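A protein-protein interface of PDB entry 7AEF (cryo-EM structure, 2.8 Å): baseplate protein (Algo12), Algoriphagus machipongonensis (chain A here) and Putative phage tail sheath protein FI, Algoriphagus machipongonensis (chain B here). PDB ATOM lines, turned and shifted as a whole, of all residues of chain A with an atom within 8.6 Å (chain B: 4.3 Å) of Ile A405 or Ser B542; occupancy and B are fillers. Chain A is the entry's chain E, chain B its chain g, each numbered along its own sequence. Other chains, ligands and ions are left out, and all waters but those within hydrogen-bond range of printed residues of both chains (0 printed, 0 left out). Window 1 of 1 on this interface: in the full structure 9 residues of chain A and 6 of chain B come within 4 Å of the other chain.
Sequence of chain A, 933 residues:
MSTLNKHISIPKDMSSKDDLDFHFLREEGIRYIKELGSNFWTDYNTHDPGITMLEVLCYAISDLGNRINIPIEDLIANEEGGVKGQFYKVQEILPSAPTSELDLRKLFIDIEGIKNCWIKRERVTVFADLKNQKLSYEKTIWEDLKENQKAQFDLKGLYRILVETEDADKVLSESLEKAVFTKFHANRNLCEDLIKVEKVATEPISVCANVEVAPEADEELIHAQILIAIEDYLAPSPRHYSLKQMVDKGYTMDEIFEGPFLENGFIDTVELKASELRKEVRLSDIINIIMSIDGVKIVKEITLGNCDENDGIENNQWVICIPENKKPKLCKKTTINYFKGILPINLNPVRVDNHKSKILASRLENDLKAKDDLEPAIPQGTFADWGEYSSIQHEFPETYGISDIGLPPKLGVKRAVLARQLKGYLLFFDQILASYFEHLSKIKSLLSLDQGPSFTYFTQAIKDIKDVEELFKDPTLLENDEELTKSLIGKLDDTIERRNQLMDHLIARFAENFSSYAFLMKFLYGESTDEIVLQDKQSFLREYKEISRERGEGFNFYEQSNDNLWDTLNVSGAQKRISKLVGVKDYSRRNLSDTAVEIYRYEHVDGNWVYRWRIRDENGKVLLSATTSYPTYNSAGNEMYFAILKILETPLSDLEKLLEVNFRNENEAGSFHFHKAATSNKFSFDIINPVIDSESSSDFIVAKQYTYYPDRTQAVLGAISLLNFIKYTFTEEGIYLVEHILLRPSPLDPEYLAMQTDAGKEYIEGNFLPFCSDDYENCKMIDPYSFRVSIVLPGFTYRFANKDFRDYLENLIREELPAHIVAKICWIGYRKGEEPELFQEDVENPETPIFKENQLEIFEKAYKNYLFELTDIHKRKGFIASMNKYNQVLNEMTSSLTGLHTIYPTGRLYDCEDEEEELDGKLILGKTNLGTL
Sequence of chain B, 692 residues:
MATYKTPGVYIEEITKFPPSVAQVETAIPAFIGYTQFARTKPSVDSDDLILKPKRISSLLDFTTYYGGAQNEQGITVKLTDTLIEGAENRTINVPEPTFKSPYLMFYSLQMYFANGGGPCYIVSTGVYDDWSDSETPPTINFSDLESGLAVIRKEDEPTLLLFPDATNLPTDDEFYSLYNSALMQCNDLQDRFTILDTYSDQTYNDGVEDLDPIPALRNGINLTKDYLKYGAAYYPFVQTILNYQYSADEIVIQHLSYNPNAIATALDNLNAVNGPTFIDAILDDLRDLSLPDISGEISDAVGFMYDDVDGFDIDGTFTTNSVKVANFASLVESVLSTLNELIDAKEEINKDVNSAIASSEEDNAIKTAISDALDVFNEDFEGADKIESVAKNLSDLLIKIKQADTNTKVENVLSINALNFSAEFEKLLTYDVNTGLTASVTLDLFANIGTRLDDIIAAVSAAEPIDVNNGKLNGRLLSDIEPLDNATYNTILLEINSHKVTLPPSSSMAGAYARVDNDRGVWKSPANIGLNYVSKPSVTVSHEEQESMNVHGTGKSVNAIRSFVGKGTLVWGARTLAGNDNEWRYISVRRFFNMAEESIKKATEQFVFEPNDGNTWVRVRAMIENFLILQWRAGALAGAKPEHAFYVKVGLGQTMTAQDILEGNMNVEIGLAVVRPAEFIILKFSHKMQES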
ATOM      1  N   HIS A 394     -28.998  10.230  16.812  1.00  0.00           N
ATOM      2  CA  HIS A 394     -27.794   9.447  17.019  1.00  0.00           C
ATOM      3  C   HIS A 394     -27.466   8.572  15.827  1.00  0.00           C
ATOM      4  O   HIS A 394     -26.442   7.890  15.835  1.00  0.00           O
ATOM      5  CB  HIS A 394     -27.940   8.580  18.262  1.00  0.00           C
ATOM      6  CG  HIS A 394     -27.951   9.357  19.526  1.00  0.00           C
ATOM      7  ND1 HIS A 394     -26.831  10.002  19.992  1.00  0.00           N
ATOM      8  CD2 HIS A 394     -28.935   9.613  20.415  1.00  0.00           C
ATOM      9  CE1 HIS A 394     -27.123  10.623  21.118  1.00  0.00           C
ATOM     10  NE2 HIS A 394     -28.394  10.409  21.394  1.00  0.00           N
ATOM     11  N   PRO A 397     -24.121  10.934  10.799  1.00  0.00           N
ATOM     12  CA  PRO A 397     -22.669  11.107  10.983  1.00  0.00           C
ATOM     13  C   PRO A 397     -22.172  12.365  11.733  1.00  0.00           C
ATOM     14  O   PRO A 397     -22.849  13.398  11.943  1.00  0.00           O
ATOM     15  CB  PRO A 397     -22.142  11.066   9.545  1.00  0.00           C
ATOM     16  CG  PRO A 397     -23.194  10.296   8.792  1.00  0.00           C
ATOM     17  CD  PRO A 397     -24.472  10.807   9.378  1.00  0.00           C
ATOM     18  N   GLU A 398     -20.908  12.236  12.148  1.00  0.00           N
ATOM     19  CA  GLU A 398     -20.273  13.272  12.943  1.00  0.00           C
ATOM     20  C   GLU A 398     -20.249  14.564  12.147  1.00  0.00           C
ATOM     21  O   GLU A 398     -20.409  15.640  12.721  1.00  0.00           O
ATOM     22  CB  GLU A 398     -18.844  12.848  13.254  1.00  0.00           C
ATOM     23  CG  GLU A 398     -18.741  11.647  14.170  1.00  0.00           C
ATOM     24  CD  GLU A 398     -17.306  11.286  14.507  1.00  0.00           C
ATOM     25  OE1 GLU A 398     -17.091  10.252  15.175  1.00  0.00           O
ATOM     26  OE2 GLU A 398     -16.389  11.995  14.041  1.00  0.00           O
ATOM     27  N   THR A 399     -20.106  14.451  10.818  1.00  0.00           N
ATOM     28  CA  THR A 399     -20.051  15.633   9.967  1.00  0.00           C
ATOM     29  C   THR A 399     -21.245  16.549  10.203  1.00  0.00           C
ATOM     30  O   THR A 399     -21.062  17.767  10.313  1.00  0.00           O
ATOM     31  CB  THR A 399     -19.960  15.244   8.485  1.00  0.00           C
ATOM     32  OG1 THR A 399     -19.838  16.437   7.707  1.00  0.00           O
ATOM     33  CG2 THR A 399     -21.170  14.454   8.006  1.00  0.00           C
ATOM     34  N   GLY A 401     -22.823  17.146  12.953  1.00  0.00           N
ATOM     35  CA  GLY A 401     -22.589  17.915  14.172  1.00  0.00           C
ATOM     36  C   GLY A 401     -23.648  17.791  15.242  1.00  0.00           C
ATOM     37  O   GLY A 401     -23.597  18.548  16.215  1.00  0.00           O
ATOM     38  N   ILE A 402     -24.586  16.852  15.106  1.00  0.00           N
ATOM     39  CA  ILE A 402     -25.691  16.691  16.055  1.00  0.00           C
ATOM     40  C   ILE A 402     -25.488  15.482  16.974  1.00  0.00           C
ATOM     41  O   ILE A 402     -26.456  14.977  17.530  1.00  0.00           O
ATOM     42  CB  ILE A 402     -27.057  16.631  15.342  1.00  0.00           C
ATOM     43  CG1 ILE A 402     -27.132  15.471  14.352  1.00  0.00           C
ATOM     44  CG2 ILE A 402     -27.344  17.944  14.647  1.00  0.00           C
ATOM     45  CD1 ILE A 402     -28.473  15.290  13.734  1.00  0.00           C
ATOM     46  N   SER A 403     -24.248  15.021  17.152  1.00  0.00           N
ATOM     47  CA  SER A 403     -23.951  13.863  17.990  1.00  0.00           C
ATOM     48  C   SER A 403     -23.289  14.300  19.296  1.00  0.00           C
ATOM     49  O   SER A 403     -22.899  15.455  19.461  1.00  0.00           O
ATOM     50  CB  SER A 403     -23.042  12.883  17.259  1.00  0.00           C
ATOM     51  OG  SER A 403     -21.746  13.407  17.158  1.00  0.00           O
ATOM     52  N   ASP A 404     -23.113  13.343  20.212  1.00  0.00           N
ATOM     53  CA  ASP A 404     -22.532  13.613  21.538  1.00  0.00           C
ATOM     54  C   ASP A 404     -21.141  14.220  21.565  1.00  0.00           C
ATOM     55  O   ASP A 404     -20.805  14.919  22.524  1.00  0.00           O
ATOM     56  CB  ASP A 404     -22.471  12.350  22.375  1.00  0.00           C
ATOM     57  CG  ASP A 404     -23.793  11.949  22.907  1.00  0.00           C
ATOM     58  OD1 ASP A 404     -24.710  12.763  22.916  1.00  0.00           O
ATOM     59  OD2 ASP A 404     -23.905  10.844  23.404  1.00  0.00           O
ATOM     60  N   ILE A 405     -20.298  13.952  20.575  1.00  0.00           N
ATOM     61  CA  ILE A 405     -18.952  14.503  20.651  1.00  0.00           C
ATOM     62  C   ILE A 405     -18.875  15.924  20.137  1.00  0.00           C
ATOM     63  O   ILE A 405     -17.798  16.529  20.166  1.00  0.00           O
ATOM     64  CB  ILE A 405     -17.954  13.608  19.898  1.00  0.00           C
ATOM     65  CG1 ILE A 405     -18.280  13.593  18.405  1.00  0.00           C
ATOM     66  CG2 ILE A 405     -17.984  12.226  20.507  1.00  0.00           C
ATOM     67  CD1 ILE A 405     -17.228  12.964  17.553  1.00  0.00           C
ATOM     68  N   GLY A 406     -19.980  16.470  19.654  1.00  0.00           N
ATOM     69  CA  GLY A 406     -19.986  17.829  19.175  1.00  0.00           C
ATOM     70  C   GLY A 406     -19.327  18.001  17.822  1.00  0.00           C
ATOM     71  O   GLY A 406     -19.324  17.114  16.975  1.00  0.00           O
ATOM     72  N   LEU A 407     -18.798  19.202  17.620  1.00  0.00           N
ATOM     73  CA  LEU A 407     -18.232  19.667  16.378  1.00  0.00           C
ATOM     74  C   LEU A 407     -16.955  20.440  16.726  1.00  0.00           C
ATOM     75  O   LEU A 407     -17.004  21.282  17.616  1.00  0.00           O
ATOM     76  CB  LEU A 407     -19.288  20.570  15.752  1.00  0.00           C
ATOM     77  CG  LEU A 407     -19.037  21.192  14.416  1.00  0.00           C
ATOM     78  CD1 LEU A 407     -19.064  20.114  13.334  1.00  0.00           C
ATOM     79  CD2 LEU A 407     -20.092  22.245  14.188  1.00  0.00           C
ATOM     80  N   PRO A 408     -15.812  20.167  16.092  1.00  0.00           N
ATOM     81  CA  PRO A 408     -14.528  20.869  16.374  1.00  0.00           C
ATOM     82  C   PRO A 408     -14.606  22.390  16.260  1.00  0.00           C
ATOM     83  O   PRO A 408     -15.072  22.898  15.239  1.00  0.00           O
ATOM     84  CB  PRO A 408     -13.616  20.308  15.277  1.00  0.00           C
ATOM     85  CG  PRO A 408     -14.182  18.967  14.972  1.00  0.00           C
ATOM     86  CD  PRO A 408     -15.664  19.109  15.099  1.00  0.00           C
ATOM     87  N   PRO A 409     -14.100  23.126  17.267  1.00  0.00           N
ATOM     88  CA  PRO A 409     -14.059  24.607  17.305  1.00  0.00           C
ATOM     89  C   PRO A 409     -13.523  25.309  16.078  1.00  0.00           C
ATOM     90  O   PRO A 409     -14.023  26.376  15.709  1.00  0.00           O
ATOM     91  CB  PRO A 409     -13.138  24.854  18.504  1.00  0.00           C
ATOM     92  CG  PRO A 409     -13.395  23.687  19.393  1.00  0.00           C
ATOM     93  CD  PRO A 409     -13.584  22.521  18.492  1.00  0.00           C
ATOM     94  N   LYS A 423     -31.097  20.340  14.896  1.00  0.00           N
ATOM     95  CA  LYS A 423     -31.657  19.615  16.037  1.00  0.00           C
ATOM     96  C   LYS A 423     -33.106  19.989  16.260  1.00  0.00           C
ATOM     97  O   LYS A 423     -33.952  19.114  16.473  1.00  0.00           O
ATOM     98  CB  LYS A 423     -30.894  19.907  17.319  1.00  0.00           C
ATOM     99  CG  LYS A 423     -29.533  19.346  17.362  1.00  0.00           C
ATOM    100  CD  LYS A 423     -28.845  19.669  18.651  1.00  0.00           C
ATOM    101  CE  LYS A 423     -27.434  19.174  18.616  1.00  0.00           C
ATOM    102  NZ  LYS A 423     -26.723  19.446  19.873  1.00  0.00           N
ATOM    103  N   LYS A 466     -28.407  16.363  23.977  1.00  0.00           N
ATOM    104  CA  LYS A 466     -27.633  17.183  24.891  1.00  0.00           C
ATOM    105  C   LYS A 466     -28.168  18.604  25.141  1.00  0.00           C
ATOM    106  O   LYS A 466     -27.960  19.133  26.233  1.00  0.00           O
ATOM    107  CB  LYS A 466     -26.193  17.290  24.432  1.00  0.00           C
ATOM    108  CG  LYS A 466     -25.378  15.988  24.472  1.00  0.00           C
ATOM    109  CD  LYS A 466     -25.075  15.581  25.938  1.00  0.00           C
ATOM    110  CE  LYS A 466     -24.165  14.356  25.986  1.00  0.00           C
ATOM    111  NZ  LYS A 466     -24.841  13.078  25.689  1.00  0.00           N
ATOM    112  N   THR B 540     -16.068   9.175  27.852  1.00  0.00           N
ATOM    113  CA  THR B 540     -16.031   9.683  26.486  1.00  0.00           C
ATOM    114  C   THR B 540     -15.588  11.137  26.487  1.00  0.00           C
ATOM    115  O   THR B 540     -16.143  11.958  27.216  1.00  0.00           O
ATOM    116  CB  THR B 540     -17.400   9.542  25.815  1.00  0.00           C
ATOM    117  OG1 THR B 540     -17.746   8.158  25.755  1.00  0.00           O
ATOM    118  CG2 THR B 540     -17.373  10.100  24.411  1.00  0.00           C
ATOM    119  N   VAL B 541     -14.595  11.454  25.673  1.00  0.00           N
ATOM    120  CA  VAL B 541     -14.043  12.796  25.616  1.00  0.00           C
ATOM    121  C   VAL B 541     -14.485  13.473  24.321  1.00  0.00           C
ATOM    122  O   VAL B 541     -14.176  12.977  23.237  1.00  0.00           O
ATOM    123  CB  VAL B 541     -12.510  12.722  25.700  1.00  0.00           C
ATOM    124  CG1 VAL B 541     -11.922  14.090  25.651  1.00  0.00           C
ATOM    125  CG2 VAL B 541     -12.085  12.004  26.982  1.00  0.00           C
ATOM    126  N   SER B 542     -15.187  14.602  24.429  1.00  0.00           N
ATOM    127  CA  SER B 542     -15.726  15.346  23.291  1.00  0.00           C
ATOM    128  C   SER B 542     -14.647  16.130  22.570  1.00  0.00           C
ATOM    129  O   SER B 542     -13.564  16.335  23.107  1.00  0.00           O
ATOM    130  CB  SER B 542     -16.763  16.334  23.760  1.00  0.00           C
ATOM    131  OG  SER B 542     -16.149  17.366  24.495  1.00  0.00           O
ATOM    132  N   HIS B 543     -14.964  16.634  21.371  1.00  0.00           N
ATOM    133  CA  HIS B 543     -13.995  17.425  20.617  1.00  0.00           C
ATOM    134  C   HIS B 543     -13.629  18.716  21.313  1.00  0.00           C
ATOM    135  O   HIS B 543     -12.464  19.128  21.278  1.00  0.00           O
ATOM    136  CB  HIS B 543     -14.515  17.716  19.219  1.00  0.00           C
ATOM    137  CG  HIS B 543     -14.327  16.585  18.270  1.00  0.00           C
ATOM    138  ND1 HIS B 543     -15.158  16.361  17.206  1.00  0.00           N
ATOM    139  CD2 HIS B 543     -13.363  15.638  18.201  1.00  0.00           C
ATOM    140  CE1 HIS B 543     -14.726  15.314  16.530  1.00  0.00           C
ATOM    141  NE2 HIS B 543     -13.635  14.856  17.114  1.00  0.00           N
ATOM    142  N   GLU B 544     -14.595  19.330  21.985  1.00  0.00           N
ATOM    143  CA  GLU B 544     -14.336  20.566  22.688  1.00  0.00           C
ATOM    144  C   GLU B 544     -13.276  20.361  23.742  1.00  0.00           C
ATOM    145  O   GLU B 544     -12.408  21.213  23.948  1.00  0.00           O
ATOM    146  CB  GLU B 544     -15.621  21.102  23.329  1.00  0.00           C
ATOM    147  CG  GLU B 544     -15.476  22.455  24.007  1.00  0.00           C
ATOM    148  CD  GLU B 544     -15.098  23.555  23.036  1.00  0.00           C
ATOM    149  OE1 GLU B 544     -15.024  23.299  21.816  1.00  0.00           O
ATOM    150  OE2 GLU B 544     -14.903  24.705  23.483  1.00  0.00           O
ATOM    151  N   GLU B 545     -13.331  19.216  24.404  1.00  0.00           N
ATOM    152  CA  GLU B 545     -12.351  18.887  25.417  1.00  0.00           C
ATOM    153  C   GLU B 545     -11.026  18.498  24.815  1.00  0.00           C
ATOM    154  O   GLU B 545      -9.984  18.973  25.270  1.00  0.00           O
ATOM    155  CB  GLU B 545     -12.855  17.777  26.328  1.00  0.00           C
ATOM    156  CG  GLU B 545     -11.904  17.497  27.488  1.00  0.00           C
ATOM    157  CD  GLU B 545     -12.432  16.515  28.473  1.00  0.00           C
ATOM    158  OE1 GLU B 545     -13.568  16.112  28.344  1.00  0.00           O
ATOM    159  OE2 GLU B 545     -11.712  16.151  29.380  1.00  0.00           O
ATOM    160  N   GLN B 546     -11.072  17.701  23.759  1.00  0.00           N
ATOM    161  CA  GLN B 546      -9.881  17.160  23.142  1.00  0.00           C
ATOM    162  C   GLN B 546      -8.926  18.224  22.629  1.00  0.00           C
ATOM    163  O   GLN B 546      -7.723  18.017  22.651  1.00  0.00           O
ATOM    164  CB  GLN B 546     -10.268  16.208  22.027  1.00  0.00           C
ATOM    165  CG  GLN B 546      -9.106  15.376  21.574  1.00  0.00           C
ATOM    166  CD  GLN B 546      -9.525  14.214  20.739  1.00  0.00           C
ATOM    167  OE1 GLN B 546     -10.710  13.918  20.618  1.00  0.00           O
ATOM    168  NE2 GLN B 546      -8.552  13.535  20.157  1.00  0.00           N
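O of Ile A405 is in hydrogen-bond range of N of His B543.
Ser B542 touches Ile A405. Pro A408 touches His B543. Pro A409 touches Glu B544 (CG to OE1, 2.9 Å).
Of chain B, only Ser B542 and His B543 come within 4 Å of Ile A405. Ser B542 touches one residue of chain A. Of the printed residues of chain B, Pro A409 touches Glu B544 (2.9 Å). Printed residues of chain A within 4 Å of His B543: Ile A405 (3.1 Å) and Pro A408 (3.5 Å).
Hydrophobic or aromatic side chains of chain B that line the printed part of chain A: His B543.
The backbone NH (N) of Glu B545 sits at hydrogen-bond distance from the side-chain hydroxyl (OG) of Ser B542, at 3.4 Å.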
